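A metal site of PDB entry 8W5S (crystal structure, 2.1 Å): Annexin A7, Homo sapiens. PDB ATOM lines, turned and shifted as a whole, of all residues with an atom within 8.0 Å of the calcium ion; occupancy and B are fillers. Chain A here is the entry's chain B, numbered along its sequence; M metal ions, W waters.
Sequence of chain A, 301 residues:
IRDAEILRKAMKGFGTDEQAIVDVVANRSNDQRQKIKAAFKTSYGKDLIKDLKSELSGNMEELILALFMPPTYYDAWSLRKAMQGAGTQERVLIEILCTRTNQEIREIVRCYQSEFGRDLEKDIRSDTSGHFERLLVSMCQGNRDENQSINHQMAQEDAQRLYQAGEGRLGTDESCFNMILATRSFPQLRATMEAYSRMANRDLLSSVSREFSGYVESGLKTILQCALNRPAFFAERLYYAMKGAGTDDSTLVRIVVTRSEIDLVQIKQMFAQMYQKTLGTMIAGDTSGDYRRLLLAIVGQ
The backbone carbonyl oxygen (O) of Glu 211 is in hydrogen-bond range of the side-chain hydroxyl (OG1) of Thr 172 (3.2 Å).
The side-chain carboxylate (OE2) of Glu 211 sits close to the backbone NH (N) of Glu 167 (3.4 Å).
The calcium ion is bound by O of Gly 166, water W1, O of Gly 171, water W2, OE1 of Glu 211, O of Arg 169 and OE2 of Glu 211.
Four residues have an atom within 4 Å of the calcium ion: Gly 166, Arg 169, Gly 171 and Glu 211.
Along chain A the residues within 4 Å of the calcium ion span positions 166 to 211.
The nearest printed residue that does not touch the calcium ion is Thr 172 (4.1 Å).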
ATOM      1  N   TYR A 163     -14.535   3.597 -20.252  1.00  0.00           N
ATOM      2  CA  TYR A 163     -13.371   4.142 -20.939  1.00  0.00           C
ATOM      3  C   TYR A 163     -12.118   4.042 -20.071  1.00  0.00           C
ATOM      4  O   TYR A 163     -11.111   3.475 -20.488  1.00  0.00           O
ATOM      5  CB  TYR A 163     -13.622   5.595 -21.347  1.00  0.00           C
ATOM      6  CG  TYR A 163     -12.727   6.041 -22.487  1.00  0.00           C
ATOM      7  CD1 TYR A 163     -13.217   6.152 -23.774  1.00  0.00           C
ATOM      8  CD2 TYR A 163     -11.383   6.340 -22.267  1.00  0.00           C
ATOM      9  CE1 TYR A 163     -12.397   6.549 -24.821  1.00  0.00           C
ATOM     10  CE2 TYR A 163     -10.564   6.737 -23.300  1.00  0.00           C
ATOM     11  CZ  TYR A 163     -11.077   6.844 -24.581  1.00  0.00           C
ATOM     12  OH  TYR A 163     -10.275   7.241 -25.614  1.00  0.00           O
ATOM     13  N   GLN A 164     -12.185   4.575 -18.852  1.00  0.00           N
ATOM     14  CA  GLN A 164     -11.049   4.516 -17.946  1.00  0.00           C
ATOM     15  C   GLN A 164     -10.701   3.098 -17.524  1.00  0.00           C
ATOM     16  O   GLN A 164      -9.639   2.879 -16.930  1.00  0.00           O
ATOM     17  CB  GLN A 164     -11.306   5.370 -16.710  1.00  0.00           C
ATOM     18  CG  GLN A 164     -10.458   6.624 -16.623  1.00  0.00           C
ATOM     19  CD  GLN A 164      -9.054   6.354 -16.084  1.00  0.00           C
ATOM     20  OE1 GLN A 164      -8.788   5.294 -15.511  1.00  0.00           O
ATOM     21  NE2 GLN A 164      -8.158   7.317 -16.265  1.00  0.00           N
ATOM     22  N   ALA A 165     -11.572   2.124 -17.817  1.00  0.00           N
ATOM     23  CA  ALA A 165     -11.321   0.729 -17.476  1.00  0.00           C
ATOM     24  C   ALA A 165     -10.606  -0.042 -18.574  1.00  0.00           C
ATOM     25  O   ALA A 165     -10.213  -1.191 -18.348  1.00  0.00           O
ATOM     26  CB  ALA A 165     -12.633   0.017 -17.137  1.00  0.00           C
ATOM     27  N   GLY A 166     -10.435   0.556 -19.747  1.00  0.00           N
ATOM     28  CA  GLY A 166      -9.767  -0.126 -20.836  1.00  0.00           C
ATOM     29  C   GLY A 166      -9.027   0.803 -21.775  1.00  0.00           C
ATOM     30  O   GLY A 166      -7.786   0.866 -21.737  1.00  0.00           O
ATOM     31  N   GLU A 167      -9.768   1.512 -22.629  1.00  0.00           N
ATOM     32  CA  GLU A 167      -9.135   2.358 -23.630  1.00  0.00           C
ATOM     33  C   GLU A 167      -8.288   3.459 -22.997  1.00  0.00           C
ATOM     34  O   GLU A 167      -7.217   3.788 -23.498  1.00  0.00           O
ATOM     35  CB  GLU A 167     -10.203   2.974 -24.548  1.00  0.00           C
ATOM     36  CG  GLU A 167     -10.950   1.970 -25.396  1.00  0.00           C
ATOM     37  CD  GLU A 167     -10.349   1.816 -26.788  1.00  0.00           C
ATOM     38  OE1 GLU A 167      -9.156   2.143 -26.940  1.00  0.00           O
ATOM     39  OE2 GLU A 167     -11.056   1.357 -27.705  1.00  0.00           O
ATOM     40  N   GLY A 168      -8.775   4.026 -21.893  1.00  0.00           N
ATOM     41  CA  GLY A 168      -8.079   5.140 -21.277  1.00  0.00           C
ATOM     42  C   GLY A 168      -7.103   4.752 -20.187  1.00  0.00           C
ATOM     43  O   GLY A 168      -6.752   5.579 -19.351  1.00  0.00           O
ATOM     44  N   ARG A 169      -6.640   3.503 -20.197  1.00  0.00           N
ATOM     45  CA  ARG A 169      -5.773   3.036 -19.127  1.00  0.00           C
ATOM     46  C   ARG A 169      -4.843   1.948 -19.632  1.00  0.00           C
ATOM     47  O   ARG A 169      -5.089   1.310 -20.660  1.00  0.00           O
ATOM     48  CB  ARG A 169      -6.587   2.515 -17.932  1.00  0.00           C
ATOM     49  CG  ARG A 169      -7.009   1.060 -18.073  1.00  0.00           C
ATOM     50  CD  ARG A 169      -7.616   0.534 -16.783  1.00  0.00           C
ATOM     51  NE  ARG A 169      -6.909  -0.629 -16.269  1.00  0.00           N
ATOM     52  CZ  ARG A 169      -6.798  -0.929 -14.985  1.00  0.00           C
ATOM     53  NH1 ARG A 169      -7.366  -0.171 -14.054  1.00  0.00           N
ATOM     54  NH2 ARG A 169      -6.113  -2.006 -14.624  1.00  0.00           N
ATOM     55  N   LEU A 170      -3.760   1.741 -18.889  1.00  0.00           N
ATOM     56  CA  LEU A 170      -2.886   0.605 -19.131  1.00  0.00           C
ATOM     57  C   LEU A 170      -3.573  -0.688 -18.704  1.00  0.00           C
ATOM     58  O   LEU A 170      -4.344  -0.708 -17.739  1.00  0.00           O
ATOM     59  CB  LEU A 170      -1.566   0.769 -18.375  1.00  0.00           C
ATOM     60  CG  LEU A 170      -0.464   1.580 -19.055  1.00  0.00           C
ATOM     61  CD1 LEU A 170       0.721   1.743 -18.130  1.00  0.00           C
ATOM     62  CD2 LEU A 170      -0.053   0.921 -20.354  1.00  0.00           C
ATOM     63  N   GLY A 171      -3.293  -1.766 -19.426  1.00  0.00           N
ATOM     64  CA  GLY A 171      -3.961  -3.016 -19.143  1.00  0.00           C
ATOM     65  C   GLY A 171      -5.455  -2.890 -19.343  1.00  0.00           C
ATOM     66  O   GLY A 171      -5.931  -2.175 -20.228  1.00  0.00           O
ATOM     67  N   THR A 172      -6.221  -3.582 -18.493  1.00  0.00           N
ATOM     68  CA  THR A 172      -7.670  -3.539 -18.561  1.00  0.00           C
ATOM     69  C   THR A 172      -8.241  -3.884 -17.187  1.00  0.00           C
ATOM     70  O   THR A 172      -7.821  -4.866 -16.573  1.00  0.00           O
ATOM     71  CB  THR A 172      -8.224  -4.501 -19.607  1.00  0.00           C
ATOM     72  OG1 THR A 172      -7.537  -4.312 -20.858  1.00  0.00           O
ATOM     73  CG2 THR A 172      -9.708  -4.281 -19.818  1.00  0.00           C
ATOM     74  N   ASP A 173      -9.178  -3.063 -16.704  1.00  0.00           N
ATOM     75  CA  ASP A 173      -9.909  -3.373 -15.483  1.00  0.00           C
ATOM     76  C   ASP A 173     -11.074  -4.270 -15.876  1.00  0.00           C
ATOM     77  O   ASP A 173     -12.215  -3.826 -16.093  1.00  0.00           O
ATOM     78  CB  ASP A 173     -10.382  -2.103 -14.788  1.00  0.00           C
ATOM     79  CG  ASP A 173     -11.212  -2.384 -13.549  1.00  0.00           C
ATOM     80  OD1 ASP A 173     -11.112  -3.505 -13.004  1.00  0.00           O
ATOM     81  OD2 ASP A 173     -11.953  -1.486 -13.116  1.00  0.00           O
ATOM     82  N   PHE A 177     -15.888  -3.984 -16.655  1.00  0.00           N
ATOM     83  CA  PHE A 177     -16.737  -4.456 -17.736  1.00  0.00           C
ATOM     84  C   PHE A 177     -17.711  -5.521 -17.254  1.00  0.00           C
ATOM     85  O   PHE A 177     -18.871  -5.548 -17.668  1.00  0.00           O
ATOM     86  CB  PHE A 177     -15.880  -4.992 -18.885  1.00  0.00           C
ATOM     87  CG  PHE A 177     -15.298  -3.928 -19.770  1.00  0.00           C
ATOM     88  CD1 PHE A 177     -14.194  -3.198 -19.349  1.00  0.00           C
ATOM     89  CD2 PHE A 177     -15.848  -3.648 -21.004  1.00  0.00           C
ATOM     90  CE1 PHE A 177     -13.658  -2.224 -20.152  1.00  0.00           C
ATOM     91  CE2 PHE A 177     -15.312  -2.663 -21.815  1.00  0.00           C
ATOM     92  CZ  PHE A 177     -14.209  -1.944 -21.386  1.00  0.00           C
ATOM     93  N   SER A 207     -13.960  -1.536 -28.482  1.00  0.00           N
ATOM     94  CA  SER A 207     -13.113  -1.467 -27.296  1.00  0.00           C
ATOM     95  C   SER A 207     -13.025  -2.808 -26.585  1.00  0.00           C
ATOM     96  O   SER A 207     -11.959  -3.178 -26.083  1.00  0.00           O
ATOM     97  CB  SER A 207     -13.645  -0.397 -26.337  1.00  0.00           C
ATOM     98  OG  SER A 207     -13.923   0.809 -27.024  1.00  0.00           O
ATOM     99  N   ARG A 210     -10.806  -4.830 -28.561  1.00  0.00           N
ATOM    100  CA  ARG A 210      -9.458  -4.298 -28.423  1.00  0.00           C
ATOM    101  C   ARG A 210      -8.876  -4.533 -27.029  1.00  0.00           C
ATOM    102  O   ARG A 210      -7.663  -4.719 -26.908  1.00  0.00           O
ATOM    103  CB  ARG A 210      -9.463  -2.797 -28.744  1.00  0.00           C
ATOM    104  CG  ARG A 210      -9.386  -2.497 -30.237  1.00  0.00           C
ATOM    105  CD  ARG A 210     -10.308  -1.360 -30.633  1.00  0.00           C
ATOM    106  NE  ARG A 210      -9.960  -0.090 -30.010  1.00  0.00           N
ATOM    107  CZ  ARG A 210      -8.880   0.629 -30.296  1.00  0.00           C
ATOM    108  NH1 ARG A 210      -7.995   0.217 -31.189  1.00  0.00           N
ATOM    109  NH2 ARG A 210      -8.681   1.791 -29.670  1.00  0.00           N
ATOM    110  N   GLU A 211      -9.706  -4.542 -25.994  1.00  0.00           N
ATOM    111  CA  GLU A 211      -9.229  -4.657 -24.621  1.00  0.00           C
ATOM    112  C   GLU A 211      -9.305  -6.065 -24.051  1.00  0.00           C
ATOM    113  O   GLU A 211      -8.688  -6.321 -23.016  1.00  0.00           O
ATOM    114  CB  GLU A 211     -10.002  -3.703 -23.710  1.00  0.00           C
ATOM    115  CG  GLU A 211      -9.758  -2.242 -24.004  1.00  0.00           C
ATOM    116  CD  GLU A 211      -8.403  -1.772 -23.516  1.00  0.00           C
ATOM    117  OE1 GLU A 211      -7.897  -2.346 -22.531  1.00  0.00           O
ATOM    118  OE2 GLU A 211      -7.853  -0.825 -24.113  1.00  0.00           O
ATOM    119  N   PHE A 212     -10.039  -6.972 -24.684  1.00  0.00           N
ATOM    120  CA  PHE A 212     -10.155  -8.340 -24.195  1.00  0.00           C
ATOM    121  C   PHE A 212      -9.749  -9.323 -25.280  1.00  0.00           C
ATOM    122  O   PHE A 212      -9.695  -8.984 -26.464  1.00  0.00           O
ATOM    123  CB  PHE A 212     -11.590  -8.651 -23.743  1.00  0.00           C
ATOM    124  CG  PHE A 212     -12.035  -7.875 -22.549  1.00  0.00           C
ATOM    125  CD1 PHE A 212     -11.788  -8.337 -21.269  1.00  0.00           C
ATOM    126  CD2 PHE A 212     -12.713  -6.682 -22.703  1.00  0.00           C
ATOM    127  CE1 PHE A 212     -12.197  -7.626 -20.163  1.00  0.00           C
ATOM    128  CE2 PHE A 212     -13.133  -5.955 -21.598  1.00  0.00           C
ATOM    129  CZ  PHE A 212     -12.869  -6.429 -20.324  1.00  0.00           C
HETATM  130 CA    CA M   1      -6.133  -0.609 -22.000  1.00  0.00          CA
HETATM  131  O   HOH W   1      -5.328   0.972 -23.572  1.00  0.00           O
HETATM  132  O   HOH W   2      -4.877  -2.346 -23.268  1.00  0.00           O
